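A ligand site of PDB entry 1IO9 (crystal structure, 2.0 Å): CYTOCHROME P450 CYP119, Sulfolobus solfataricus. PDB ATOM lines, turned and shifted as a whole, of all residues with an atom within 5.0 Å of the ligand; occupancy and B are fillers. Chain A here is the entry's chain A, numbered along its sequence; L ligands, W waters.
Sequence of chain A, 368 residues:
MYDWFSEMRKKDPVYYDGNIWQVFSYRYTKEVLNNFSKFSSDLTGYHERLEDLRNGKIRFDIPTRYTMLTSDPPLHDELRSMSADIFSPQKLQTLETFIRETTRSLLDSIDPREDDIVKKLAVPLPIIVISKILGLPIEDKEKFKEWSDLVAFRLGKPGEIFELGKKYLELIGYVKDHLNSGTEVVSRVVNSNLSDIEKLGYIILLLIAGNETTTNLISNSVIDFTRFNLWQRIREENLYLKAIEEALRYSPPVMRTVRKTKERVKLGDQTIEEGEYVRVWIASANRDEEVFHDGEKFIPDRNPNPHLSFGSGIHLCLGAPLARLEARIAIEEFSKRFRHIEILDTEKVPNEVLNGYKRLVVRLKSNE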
ATOM      1  N   LEU A  33      30.261 -29.286  -9.806  1.00  0.00           N
ATOM      2  CA  LEU A  33      29.541 -28.745  -8.649  1.00  0.00           C
ATOM      3  C   LEU A  33      28.859 -29.788  -7.782  1.00  0.00           C
ATOM      4  O   LEU A  33      28.662 -29.585  -6.579  1.00  0.00           O
ATOM      5  CB  LEU A  33      28.471 -27.739  -9.111  1.00  0.00           C
ATOM      6  CG  LEU A  33      28.901 -26.347  -9.589  1.00  0.00           C
ATOM      7  CD1 LEU A  33      27.673 -25.451  -9.770  1.00  0.00           C
ATOM      8  CD2 LEU A  33      29.869 -25.738  -8.590  1.00  0.00           C
ATOM      9  N   MET A  68      31.117 -23.172   6.254  1.00  0.00           N
ATOM     10  CA  MET A  68      30.568 -24.259   5.457  1.00  0.00           C
ATOM     11  C   MET A  68      30.919 -24.098   3.989  1.00  0.00           C
ATOM     12  O   MET A  68      30.912 -25.063   3.234  1.00  0.00           O
ATOM     13  CB  MET A  68      29.047 -24.346   5.610  1.00  0.00           C
ATOM     14  CG  MET A  68      28.268 -23.121   5.123  1.00  0.00           C
ATOM     15  SD  MET A  68      26.493 -23.299   5.445  1.00  0.00           S
ATOM     16  CE  MET A  68      26.306 -22.475   7.008  1.00  0.00           C
ATOM     17  N   LEU A  69      31.224 -22.877   3.583  1.00  0.00           N
ATOM     18  CA  LEU A  69      31.550 -22.607   2.188  1.00  0.00           C
ATOM     19  C   LEU A  69      32.864 -23.277   1.776  1.00  0.00           C
ATOM     20  O   LEU A  69      32.951 -23.788   0.663  1.00  0.00           O
ATOM     21  CB  LEU A  69      31.631 -21.087   1.934  1.00  0.00           C
ATOM     22  CG  LEU A  69      31.040 -20.428   0.686  1.00  0.00           C
ATOM     23  CD1 LEU A  69      32.045 -19.412   0.171  1.00  0.00           C
ATOM     24  CD2 LEU A  69      30.747 -21.440  -0.396  1.00  0.00           C
ATOM     25  N   HIS A  76      31.052 -30.244   6.347  1.00  0.00           N
ATOM     26  CA  HIS A  76      30.124 -29.340   5.666  1.00  0.00           C
ATOM     27  C   HIS A  76      28.701 -29.565   6.138  1.00  0.00           C
ATOM     28  O   HIS A  76      27.986 -28.607   6.467  1.00  0.00           O
ATOM     29  CB  HIS A  76      30.117 -29.522   4.145  1.00  0.00           C
ATOM     30  CG  HIS A  76      29.032 -28.721   3.471  1.00  0.00           C
ATOM     31  ND1 HIS A  76      27.821 -29.266   3.120  1.00  0.00           N
ATOM     32  CD2 HIS A  76      28.961 -27.401   3.173  1.00  0.00           C
ATOM     33  CE1 HIS A  76      27.035 -28.319   2.643  1.00  0.00           C
ATOM     34  NE2 HIS A  76      27.697 -27.178   2.671  1.00  0.00           N
ATOM     35  N   ARG A  80      26.166 -26.932   8.138  1.00  0.00           N
ATOM     36  CA  ARG A  80      24.950 -26.465   7.482  1.00  0.00           C
ATOM     37  C   ARG A  80      23.647 -26.769   8.213  1.00  0.00           C
ATOM     38  O   ARG A  80      22.718 -25.946   8.207  1.00  0.00           O
ATOM     39  CB  ARG A  80      24.888 -26.991   6.044  1.00  0.00           C
ATOM     40  CG  ARG A  80      23.756 -26.369   5.242  1.00  0.00           C
ATOM     41  CD  ARG A  80      24.030 -26.393   3.762  1.00  0.00           C
ATOM     42  NE  ARG A  80      22.826 -26.047   3.008  1.00  0.00           N
ATOM     43  CZ  ARG A  80      22.824 -25.498   1.794  1.00  0.00           C
ATOM     44  NH1 ARG A  80      23.953 -25.226   1.158  1.00  0.00           N
ATOM     45  NH2 ARG A  80      21.661 -25.246   1.192  1.00  0.00           N
ATOM     46  N   PHE A  87      16.128 -20.553   6.841  1.00  0.00           N
ATOM     47  CA  PHE A  87      15.741 -20.106   5.513  1.00  0.00           C
ATOM     48  C   PHE A  87      14.888 -21.235   4.938  1.00  0.00           C
ATOM     49  O   PHE A  87      15.303 -21.922   4.017  1.00  0.00           O
ATOM     50  CB  PHE A  87      16.966 -19.882   4.623  1.00  0.00           C
ATOM     51  CG  PHE A  87      18.014 -18.972   5.239  1.00  0.00           C
ATOM     52  CD1 PHE A  87      19.262 -19.470   5.588  1.00  0.00           C
ATOM     53  CD2 PHE A  87      17.744 -17.629   5.463  1.00  0.00           C
ATOM     54  CE1 PHE A  87      20.232 -18.634   6.159  1.00  0.00           C
ATOM     55  CE2 PHE A  87      18.702 -16.791   6.026  1.00  0.00           C
ATOM     56  CZ  PHE A  87      19.951 -17.298   6.372  1.00  0.00           C
ATOM     57  N   ILE A 130      18.575  -9.097   6.486  1.00  0.00           N
ATOM     58  CA  ILE A 130      19.466 -10.049   7.146  1.00  0.00           C
ATOM     59  C   ILE A 130      19.739  -9.619   8.593  1.00  0.00           C
ATOM     60  O   ILE A 130      19.883 -10.472   9.472  1.00  0.00           O
ATOM     61  CB  ILE A 130      20.806 -10.196   6.354  1.00  0.00           C
ATOM     62  CG1 ILE A 130      21.478 -11.507   6.744  1.00  0.00           C
ATOM     63  CG2 ILE A 130      21.712  -9.004   6.588  1.00  0.00           C
ATOM     64  CD1 ILE A 130      20.585 -12.721   6.564  1.00  0.00           C
ATOM     65  N   PHE A 153      33.459 -14.285  -3.039  1.00  0.00           N
ATOM     66  CA  PHE A 153      33.595 -14.327  -4.505  1.00  0.00           C
ATOM     67  C   PHE A 153      34.565 -13.304  -5.041  1.00  0.00           C
ATOM     68  O   PHE A 153      35.068 -13.447  -6.149  1.00  0.00           O
ATOM     69  CB  PHE A 153      32.232 -14.125  -5.179  1.00  0.00           C
ATOM     70  CG  PHE A 153      31.194 -15.145  -4.791  1.00  0.00           C
ATOM     71  CD1 PHE A 153      29.992 -14.743  -4.216  1.00  0.00           C
ATOM     72  CD2 PHE A 153      31.404 -16.494  -5.013  1.00  0.00           C
ATOM     73  CE1 PHE A 153      29.005 -15.675  -3.871  1.00  0.00           C
ATOM     74  CE2 PHE A 153      30.429 -17.438  -4.665  1.00  0.00           C
ATOM     75  CZ  PHE A 153      29.233 -17.012  -4.093  1.00  0.00           C
ATOM     76  N   LEU A 205      29.669 -15.163   7.701  1.00  0.00           N
ATOM     77  CA  LEU A 205      29.172 -15.772   6.456  1.00  0.00           C
ATOM     78  C   LEU A 205      27.702 -15.457   6.263  1.00  0.00           C
ATOM     79  O   LEU A 205      27.312 -14.878   5.265  1.00  0.00           O
ATOM     80  CB  LEU A 205      29.325 -17.290   6.465  1.00  0.00           C
ATOM     81  CG  LEU A 205      28.740 -18.070   5.272  1.00  0.00           C
ATOM     82  CD1 LEU A 205      29.663 -17.962   4.087  1.00  0.00           C
ATOM     83  CD2 LEU A 205      28.565 -19.531   5.626  1.00  0.00           C
ATOM     84  N   LEU A 206      26.878 -15.865   7.224  1.00  0.00           N
ATOM     85  CA  LEU A 206      25.456 -15.603   7.141  1.00  0.00           C
ATOM     86  C   LEU A 206      25.234 -14.097   6.966  1.00  0.00           C
ATOM     87  O   LEU A 206      24.291 -13.672   6.304  1.00  0.00           O
ATOM     88  CB  LEU A 206      24.764 -16.103   8.420  1.00  0.00           C
ATOM     89  CG  LEU A 206      24.670 -17.629   8.531  1.00  0.00           C
ATOM     90  CD1 LEU A 206      23.890 -18.000   9.773  1.00  0.00           C
ATOM     91  CD2 LEU A 206      23.992 -18.200   7.289  1.00  0.00           C
ATOM     92  N   ALA A 209      27.214 -13.038   3.072  1.00  0.00           N
ATOM     93  CA  ALA A 209      27.066 -13.934   1.925  1.00  0.00           C
ATOM     94  C   ALA A 209      26.087 -13.488   0.849  1.00  0.00           C
ATOM     95  O   ALA A 209      26.345 -13.671  -0.338  1.00  0.00           O
ATOM     96  CB  ALA A 209      26.690 -15.335   2.408  1.00  0.00           C
ATOM     97  N   GLY A 210      24.947 -12.913   1.235  1.00  0.00           N
ATOM     98  CA  GLY A 210      23.977 -12.516   0.225  1.00  0.00           C
ATOM     99  C   GLY A 210      23.692 -11.035   0.022  1.00  0.00           C
ATOM    100  O   GLY A 210      22.717 -10.684  -0.651  1.00  0.00           O
ATOM    101  N   THR A 213      25.430  -9.939  -3.644  1.00  0.00           N
ATOM    102  CA  THR A 213      24.826 -10.838  -4.639  1.00  0.00           C
ATOM    103  C   THR A 213      23.354 -10.508  -4.891  1.00  0.00           C
ATOM    104  O   THR A 213      22.941 -10.350  -6.033  1.00  0.00           O
ATOM    105  CB  THR A 213      24.970 -12.333  -4.197  1.00  0.00           C
ATOM    106  OG1 THR A 213      24.589 -12.469  -2.822  1.00  0.00           O
ATOM    107  CG2 THR A 213      26.408 -12.807  -4.381  1.00  0.00           C
ATOM    108  N   THR A 214      22.565 -10.409  -3.810  1.00  0.00           N
ATOM    109  CA  THR A 214      21.134 -10.100  -3.904  1.00  0.00           C
ATOM    110  C   THR A 214      20.900  -8.676  -4.452  1.00  0.00           C
ATOM    111  O   THR A 214      19.922  -8.417  -5.163  1.00  0.00           O
ATOM    112  CB  THR A 214      20.436 -10.241  -2.522  1.00  0.00           C
ATOM    113  OG1 THR A 214      20.628 -11.565  -2.012  1.00  0.00           O
ATOM    114  CG2 THR A 214      18.954  -9.974  -2.654  1.00  0.00           C
ATOM    115  N   LEU A 217      21.162  -8.916  -8.041  1.00  0.00           N
ATOM    116  CA  LEU A 217      20.007  -9.564  -8.624  1.00  0.00           C
ATOM    117  C   LEU A 217      18.933  -8.531  -8.919  1.00  0.00           C
ATOM    118  O   LEU A 217      18.357  -8.509  -9.999  1.00  0.00           O
ATOM    119  CB  LEU A 217      19.466 -10.621  -7.674  1.00  0.00           C
ATOM    120  CG  LEU A 217      18.102 -11.236  -8.016  1.00  0.00           C
ATOM    121  CD1 LEU A 217      18.119 -11.785  -9.438  1.00  0.00           C
ATOM    122  CD2 LEU A 217      17.784 -12.334  -7.004  1.00  0.00           C
ATOM    123  N   LEU A 248      17.973 -14.294 -13.298  1.00  0.00           N
ATOM    124  CA  LEU A 248      19.027 -15.023 -12.620  1.00  0.00           C
ATOM    125  C   LEU A 248      19.872 -15.794 -13.623  1.00  0.00           C
ATOM    126  O   LEU A 248      21.085 -15.861 -13.500  1.00  0.00           O
ATOM    127  CB  LEU A 248      18.432 -15.999 -11.613  1.00  0.00           C
ATOM    128  CG  LEU A 248      18.138 -15.474 -10.212  1.00  0.00           C
ATOM    129  CD1 LEU A 248      17.214 -16.443  -9.488  1.00  0.00           C
ATOM    130  CD2 LEU A 248      19.439 -15.319  -9.467  1.00  0.00           C
ATOM    131  N   PRO A 253      24.503 -12.912 -10.966  1.00  0.00           N
ATOM    132  CA  PRO A 253      25.248 -12.091  -9.993  1.00  0.00           C
ATOM    133  C   PRO A 253      26.652 -12.646  -9.683  1.00  0.00           C
ATOM    134  O   PRO A 253      27.567 -11.889  -9.374  1.00  0.00           O
ATOM    135  CB  PRO A 253      24.361 -12.093  -8.742  1.00  0.00           C
ATOM    136  CG  PRO A 253      22.997 -12.413  -9.240  1.00  0.00           C
ATOM    137  CD  PRO A 253      23.195 -13.332 -10.425  1.00  0.00           C
ATOM    138  N   VAL A 254      26.805 -13.963  -9.735  1.00  0.00           N
ATOM    139  CA  VAL A 254      28.088 -14.625  -9.506  1.00  0.00           C
ATOM    140  C   VAL A 254      28.381 -15.283 -10.850  1.00  0.00           C
ATOM    141  O   VAL A 254      27.666 -16.196 -11.270  1.00  0.00           O
ATOM    142  CB  VAL A 254      27.992 -15.717  -8.389  1.00  0.00           C
ATOM    143  CG1 VAL A 254      29.264 -16.553  -8.316  1.00  0.00           C
ATOM    144  CG2 VAL A 254      27.746 -15.057  -7.067  1.00  0.00           C
ATOM    145  N   THR A 257      32.570 -19.914 -10.079  1.00  0.00           N
ATOM    146  CA  THR A 257      32.933 -20.406  -8.752  1.00  0.00           C
ATOM    147  C   THR A 257      34.104 -21.354  -8.998  1.00  0.00           C
ATOM    148  O   THR A 257      34.343 -21.755 -10.137  1.00  0.00           O
ATOM    149  CB  THR A 257      31.760 -21.113  -8.049  1.00  0.00           C
ATOM    150  OG1 THR A 257      32.173 -21.461  -6.720  1.00  0.00           O
ATOM    151  CG2 THR A 257      31.352 -22.388  -8.790  1.00  0.00           C
ATOM    152  N   VAL A 258      34.829 -21.721  -7.950  1.00  0.00           N
ATOM    153  CA  VAL A 258      35.986 -22.601  -8.100  1.00  0.00           C
ATOM    154  C   VAL A 258      35.908 -23.899  -7.293  1.00  0.00           C
ATOM    155  O   VAL A 258      35.129 -24.014  -6.345  1.00  0.00           O
ATOM    156  CB  VAL A 258      37.288 -21.877  -7.720  1.00  0.00           C
ATOM    157  CG1 VAL A 258      37.240 -21.485  -6.267  1.00  0.00           C
ATOM    158  CG2 VAL A 258      38.487 -22.761  -7.981  1.00  0.00           C
ATOM    159  N   ARG A 259      36.735 -24.861  -7.695  1.00  0.00           N
ATOM    160  CA  ARG A 259      36.849 -26.162  -7.023  1.00  0.00           C
ATOM    161  C   ARG A 259      38.312 -26.596  -7.142  1.00  0.00           C
ATOM    162  O   ARG A 259      39.058 -26.039  -7.958  1.00  0.00           O
ATOM    163  CB  ARG A 259      35.937 -27.206  -7.682  1.00  0.00           C
ATOM    164  CG  ARG A 259      34.444 -27.010  -7.420  1.00  0.00           C
ATOM    165  CD  ARG A 259      34.085 -27.127  -5.955  1.00  0.00           C
ATOM    166  NE  ARG A 259      32.639 -27.086  -5.679  1.00  0.00           N
ATOM    167  CZ  ARG A 259      31.949 -25.966  -5.467  1.00  0.00           C
ATOM    168  NH1 ARG A 259      32.574 -24.785  -5.491  1.00  0.00           N
ATOM    169  NH2 ARG A 259      30.667 -26.032  -5.163  1.00  0.00           N
ATOM    170  N   ILE A 282      29.695 -20.398 -14.362  1.00  0.00           N
ATOM    171  CA  ILE A 282      28.256 -20.456 -14.183  1.00  0.00           C
ATOM    172  C   ILE A 282      27.527 -19.671 -15.293  1.00  0.00           C
ATOM    173  O   ILE A 282      26.538 -20.149 -15.836  1.00  0.00           O
ATOM    174  CB  ILE A 282      27.841 -19.892 -12.793  1.00  0.00           C
ATOM    175  CG1 ILE A 282      28.143 -20.930 -11.706  1.00  0.00           C
ATOM    176  CG2 ILE A 282      26.355 -19.533 -12.809  1.00  0.00           C
ATOM    177  CD1 ILE A 282      28.088 -20.387 -10.277  1.00  0.00           C
ATOM    178  N   SER A 309      22.697 -20.480 -11.154  1.00  0.00           N
ATOM    179  CA  SER A 309      23.124 -19.249 -10.512  1.00  0.00           C
ATOM    180  C   SER A 309      23.294 -19.336  -8.996  1.00  0.00           C
ATOM    181  O   SER A 309      24.037 -18.546  -8.411  1.00  0.00           O
ATOM    182  CB  SER A 309      22.164 -18.125 -10.898  1.00  0.00           C
ATOM    183  OG  SER A 309      22.083 -18.031 -12.311  1.00  0.00           O
ATOM    184  N   PHE A 310      22.618 -20.287  -8.369  1.00  0.00           N
ATOM    185  CA  PHE A 310      22.728 -20.460  -6.917  1.00  0.00           C
ATOM    186  C   PHE A 310      23.625 -21.646  -6.653  1.00  0.00           C
ATOM    187  O   PHE A 310      23.771 -22.076  -5.513  1.00  0.00           O
ATOM    188  CB  PHE A 310      21.355 -20.734  -6.322  1.00  0.00           C
ATOM    189  CG  PHE A 310      20.529 -19.516  -6.160  1.00  0.00           C
ATOM    190  CD1 PHE A 310      19.326 -19.371  -6.851  1.00  0.00           C
ATOM    191  CD2 PHE A 310      20.943 -18.484  -5.309  1.00  0.00           C
ATOM    192  CE1 PHE A 310      18.543 -18.212  -6.723  1.00  0.00           C
ATOM    193  CE2 PHE A 310      20.175 -17.331  -5.164  1.00  0.00           C
ATOM    194  CZ  PHE A 310      18.970 -17.191  -5.868  1.00  0.00           C
ATOM    195  N   GLY A 311      24.222 -22.158  -7.723  1.00  0.00           N
ATOM    196  CA  GLY A 311      25.095 -23.307  -7.626  1.00  0.00           C
ATOM    197  C   GLY A 311      24.279 -24.584  -7.772  1.00  0.00           C
ATOM    198  O   GLY A 311      23.133 -24.543  -8.232  1.00  0.00           O
ATOM    199  N   ILE A 314      25.605 -29.993  -2.803  1.00  0.00           N
ATOM    200  CA  ILE A 314      25.496 -29.753  -1.363  1.00  0.00           C
ATOM    201  C   ILE A 314      25.696 -28.293  -0.994  1.00  0.00           C
ATOM    202  O   ILE A 314      25.207 -27.856   0.042  1.00  0.00           O
ATOM    203  CB  ILE A 314      26.508 -30.635  -0.538  1.00  0.00           C
ATOM    204  CG1 ILE A 314      27.952 -30.324  -0.925  1.00  0.00           C
ATOM    205  CG2 ILE A 314      26.244 -32.111  -0.754  1.00  0.00           C
ATOM    206  CD1 ILE A 314      28.957 -30.840   0.062  1.00  0.00           C
ATOM    207  N   HIS A 315      26.393 -27.513  -1.829  1.00  0.00           N
ATOM    208  CA  HIS A 315      26.607 -26.106  -1.486  1.00  0.00           C
ATOM    209  C   HIS A 315      25.593 -25.138  -2.076  1.00  0.00           C
ATOM    210  O   HIS A 315      25.718 -23.932  -1.892  1.00  0.00           O
ATOM    211  CB  HIS A 315      28.024 -25.677  -1.873  1.00  0.00           C
ATOM    212  CG  HIS A 315      29.100 -26.370  -1.097  1.00  0.00           C
ATOM    213  ND1 HIS A 315      29.612 -25.870   0.077  1.00  0.00           N
ATOM    214  CD2 HIS A 315      29.752 -27.538  -1.331  1.00  0.00           C
ATOM    215  CE1 HIS A 315      30.540 -26.691   0.538  1.00  0.00           C
ATOM    216  NE2 HIS A 315      30.641 -27.711  -0.299  1.00  0.00           N
ATOM    217  N   LEU A 316      24.593 -25.674  -2.794  1.00  0.00           N
ATOM    218  CA  LEU A 316      23.554 -24.825  -3.394  1.00  0.00           C
ATOM    219  C   LEU A 316      23.236 -23.731  -2.386  1.00  0.00           C
ATOM    220  O   LEU A 316      22.911 -24.019  -1.231  1.00  0.00           O
ATOM    221  CB  LEU A 316      22.295 -25.660  -3.685  1.00  0.00           C
ATOM    222  CG  LEU A 316      21.467 -25.496  -4.967  1.00  0.00           C
ATOM    223  CD1 LEU A 316      20.024 -25.620  -4.582  1.00  0.00           C
ATOM    224  CD2 LEU A 316      21.693 -24.168  -5.665  1.00  0.00           C
ATOM    225  N   CYS A 317      23.345 -22.486  -2.835  1.00  0.00           N
ATOM    226  CA  CYS A 317      23.130 -21.316  -1.987  1.00  0.00           C
ATOM    227  C   CYS A 317      22.127 -21.431  -0.853  1.00  0.00           C
ATOM    228  O   CYS A 317      20.932 -21.618  -1.094  1.00  0.00           O
ATOM    229  CB  CYS A 317      22.744 -20.124  -2.837  1.00  0.00           C
ATOM    230  SG  CYS A 317      22.597 -18.638  -1.799  1.00  0.00           S
ATOM    231  N   LEU A 318      22.603 -21.288   0.385  1.00  0.00           N
ATOM    232  CA  LEU A 318      21.750 -21.365   1.587  1.00  0.00           C
ATOM    233  C   LEU A 318      20.597 -20.337   1.597  1.00  0.00           C
ATOM    234  O   LEU A 318      19.489 -20.634   2.041  1.00  0.00           O
ATOM    235  CB  LEU A 318      22.616 -21.184   2.857  1.00  0.00           C
ATOM    236  CG  LEU A 318      22.303 -21.853   4.220  1.00  0.00           C
ATOM    237  CD1 LEU A 318      22.640 -20.868   5.347  1.00  0.00           C
ATOM    238  CD2 LEU A 318      20.848 -22.285   4.328  1.00  0.00           C
ATOM    239  N   GLY A 319      20.854 -19.130   1.086  1.00  0.00           N
ATOM    240  CA  GLY A 319      19.815 -18.120   1.082  1.00  0.00           C
ATOM    241  C   GLY A 319      18.994 -17.927  -0.190  1.00  0.00           C
ATOM    242  O   GLY A 319      18.285 -16.938  -0.314  1.00  0.00           O
ATOM    243  N   ALA A 320      19.094 -18.861  -1.125  1.00  0.00           N
ATOM    244  CA  ALA A 320      18.351 -18.754  -2.384  1.00  0.00           C
ATOM    245  C   ALA A 320      16.861 -18.372  -2.225  1.00  0.00           C
ATOM    246  O   ALA A 320      16.390 -17.427  -2.844  1.00  0.00           O
ATOM    247  CB  ALA A 320      18.484 -20.056  -3.167  1.00  0.00           C
ATOM    248  N   LEU A 322      15.424 -16.920   0.193  1.00  0.00           N
ATOM    249  CA  LEU A 322      15.335 -15.589   0.788  1.00  0.00           C
ATOM    250  C   LEU A 322      15.559 -14.628  -0.356  1.00  0.00           C
ATOM    251  O   LEU A 322      14.760 -13.724  -0.604  1.00  0.00           O
ATOM    252  CB  LEU A 322      16.438 -15.395   1.841  1.00  0.00           C
ATOM    253  CG  LEU A 322      16.169 -14.508   3.062  1.00  0.00           C
ATOM    254  CD1 LEU A 322      17.423 -13.716   3.403  1.00  0.00           C
ATOM    255  CD2 LEU A 322      15.004 -13.575   2.804  1.00  0.00           C
ATOM    256  N   ALA A 323      16.667 -14.830  -1.059  1.00  0.00           N
ATOM    257  CA  ALA A 323      17.071 -14.015  -2.185  1.00  0.00           C
ATOM    258  C   ALA A 323      15.891 -13.896  -3.169  1.00  0.00           C
ATOM    259  O   ALA A 323      15.533 -12.794  -3.597  1.00  0.00           O
ATOM    260  CB  ALA A 323      18.278 -14.641  -2.873  1.00  0.00           C
HETATM  261  C1  LIG L   1      26.476 -20.234  -1.533  1.00  0.00           C
HETATM  262  C2  LIG L   1      24.938 -17.416  -5.138  1.00  0.00           C
HETATM  263  C3  LIG L   1      22.240 -14.901  -2.019  1.00  0.00           C
HETATM  264  C4  LIG L   1      24.066 -17.461   1.699  1.00  0.00           C
HETATM  265  C5  LIG L   1      26.243 -19.706  -2.844  1.00  0.00           C
HETATM  266  C6  LIG L   1      26.719 -20.285  -4.134  1.00  0.00           C
HETATM  267  C7  LIG L   1      26.363 -19.421  -5.157  1.00  0.00           C
HETATM  268  C8  LIG L   1      25.558 -18.402  -4.472  1.00  0.00           C
HETATM  269  C9  LIG L   1      26.868 -19.447  -6.616  1.00  0.00           C
HETATM  270  C10 LIG L   1      27.471 -21.610  -4.289  1.00  0.00           C
HETATM  271  C11 LIG L   1      28.974 -21.500  -4.064  1.00  0.00           C
HETATM  272  C12 LIG L   1      29.716 -22.787  -4.412  1.00  0.00           C
HETATM  273  O1  LIG L   1      29.054 -23.831  -4.589  1.00  0.00           O
HETATM  274  O2  LIG L   1      30.970 -22.768  -4.507  1.00  0.00           O
HETATM  275  C13 LIG L   1      24.150 -16.451  -4.579  1.00  0.00           C
HETATM  276  C14 LIG L   1      23.315 -15.572  -5.392  1.00  0.00           C
HETATM  277  C15 LIG L   1      22.557 -14.888  -4.500  1.00  0.00           C
HETATM  278  C16 LIG L   1      22.899 -15.331  -3.192  1.00  0.00           C
HETATM  279  C17 LIG L   1      23.313 -15.472  -6.933  1.00  0.00           C
HETATM  280  C18 LIG L   1      21.554 -13.927  -4.742  1.00  0.00           C
HETATM  281  C19 LIG L   1      20.851 -13.819  -5.945  1.00  0.00           C
HETATM  282  C20 LIG L   1      22.455 -15.434  -0.750  1.00  0.00           C
HETATM  283  C21 LIG L   1      21.743 -15.006   0.469  1.00  0.00           C
HETATM  284  C22 LIG L   1      22.328 -15.650   1.526  1.00  0.00           C
HETATM  285  C23 LIG L   1      23.367 -16.515   0.958  1.00  0.00           C
HETATM  286  C24 LIG L   1      20.561 -14.019   0.568  1.00  0.00           C
HETATM  287  C25 LIG L   1      21.881 -15.568   2.839  1.00  0.00           C
HETATM  288  C26 LIG L   1      22.699 -15.380   3.958  1.00  0.00           C
HETATM  289  C27 LIG L   1      24.918 -18.409   1.164  1.00  0.00           C
HETATM  290  C28 LIG L   1      25.636 -19.413   1.966  1.00  0.00           C
HETATM  291  C29 LIG L   1      26.236 -20.238   1.044  1.00  0.00           C
HETATM  292  C30 LIG L   1      25.948 -19.721  -0.302  1.00  0.00           C
HETATM  293  C31 LIG L   1      25.600 -19.528   3.510  1.00  0.00           C
HETATM  294  C32 LIG L   1      27.051 -21.478   1.318  1.00  0.00           C
HETATM  295  C33 LIG L   1      26.234 -22.738   1.234  1.00  0.00           C
HETATM  296  C34 LIG L   1      27.046 -23.975   1.553  1.00  0.00           C
HETATM  297  O3  LIG L   1      26.457 -24.997   1.976  1.00  0.00           O
HETATM  298  O4  LIG L   1      28.291 -23.907   1.392  1.00  0.00           O
HETATM  299  N1  LIG L   1      25.482 -18.558  -3.068  1.00  0.00           N
HETATM  300  N2  LIG L   1      23.846 -16.336  -3.242  1.00  0.00           N
HETATM  301  N3  LIG L   1      23.417 -16.409  -0.459  1.00  0.00           N
HETATM  302  N4  LIG L   1      25.126 -18.606  -0.204  1.00  0.00           N
HETATM  303 FE1  LIG L   1      24.424 -17.521  -1.707  1.00  0.00          FE
HETATM  304  O   HOH W   1      26.877 -25.222  -5.615  1.00  0.00           O
HETATM  305  O   HOH W   2      23.978 -12.155   3.833  1.00  0.00           O
HETATM  306  O   HOH W   3      25.874 -16.381  -1.636  1.00  0.00           O
HETATM  307  O   HOH W   4      31.799 -24.435  -1.922  1.00  0.00           O
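Water W4 lies within hydrogen-bond range of the backbone carbonyl oxygen of Leu 69 (2.9 Å), an oxygen (O2) of the ligand (3.2 Å) and a ring nitrogen (ND1) of His 315 (3.3 Å).
The backbone NH (N) of Cys 317 sits at hydrogen-bond distance from the backbone carbonyl oxygen (O) of Phe 310, at 2.7 Å.
N of Gly 319 sits close to SG of Cys 317, 3.4 Å away.
The side-chain sulfur (SG) of Cys 317 sits close to the backbone NH (N) of Ala 320, 3.6 Å away.
A ring nitrogen (ND1) of His 315 sits at hydrogen-bond distance from a ring nitrogen (NE2) of His 76 (3.5 Å).
O of Ile 314 sits at hydrogen-bond distance from NH1 of Arg 80, at 3.1 Å.
The guanidinium group (NH1) of Arg 80 is in hydrogen-bond range of the backbone carbonyl oxygen (O) of Leu 316, 2.9 Å away.
The side-chain hydroxyl (OG1) of Thr 213 sits close to the backbone carbonyl oxygen (O) of Gly 210 (3.4 Å).
The side-chain hydroxyl of Thr 214 is in hydrogen-bond range of the backbone carbonyl oxygen of Gly 210.
O4 of the ligand lies close to O of Met 68, at 3.4 Å.
CA of Leu 69 touches O4 of the ligand, at 3.6 Å.
Phe 153 touches the ligand (CZ to C7, 3.9 Å).
Leu 205 touches the ligand (CD2 to C31, 3.6 Å).
O of Leu 206 touches C26 of the ligand (3.3 Å).
Ala 209 touches the ligand (CB to C4, 3.5 Å).
Gly 210 touches the ligand.
OG1 of Thr 213 touches C16 of the ligand, 3.3 Å away.
OG1 of Thr 214 touches C24 of the ligand, at 3.6 Å.
Leu 217 touches the ligand (CD2 to C19, 3.6 Å).
CG of Pro 253 touches C17 of the ligand, at 3.8 Å.
CD1 of Ile 282 touches C9 of the ligand, 3.97 Å away.
Ser 309 touches the ligand.
CE2 of Phe 310 touches C15 of the ligand, 3.5 Å away.
N of Gly 311 touches C9 of the ligand (3.9 Å).
O of Ile 314 touches O3 of the ligand, at 3.7 Å.
CB of Leu 318 touches C31 of the ligand (3.5 Å).
Gly 319 touches the ligand (CA to C22, 3.6 Å).
Ala 323 touches the ligand.
Hydrophobic or aromatic side chains that line the ligand: Met 68, Leu 69, His 76, Phe 153, Leu 205, Ala 209, Leu 217, Pro 253, Ile 282, Phe 310, His 315, Leu 318 and Ala 323.
Of the 34 residues printed, 25 come within 4 Å of the ligand.
An iron atom (FE1) of the ligand is bound by the side-chain sulfur (SG) of Cys 317, 2.1 Å away.
O3 of the ligand is in hydrogen-bond range of NE2 of His 76, at 2.6 Å.
NH1 of Arg 80 is in salt-bridge range of O3 of the ligand (2.6 Å).
An oxygen (O4) of the ligand sits at hydrogen-bond distance from a ring nitrogen (ND1) of His 315, at 2.7 Å.
An oxygen (O2) of the ligand is in salt-bridge range of the guanidinium group (NH1) of Arg 259, at 2.8 Å.
An oxygen (O2) of the ligand sits at hydrogen-bond distance from the side-chain hydroxyl (OG1) of Thr 257 (2.8 Å).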
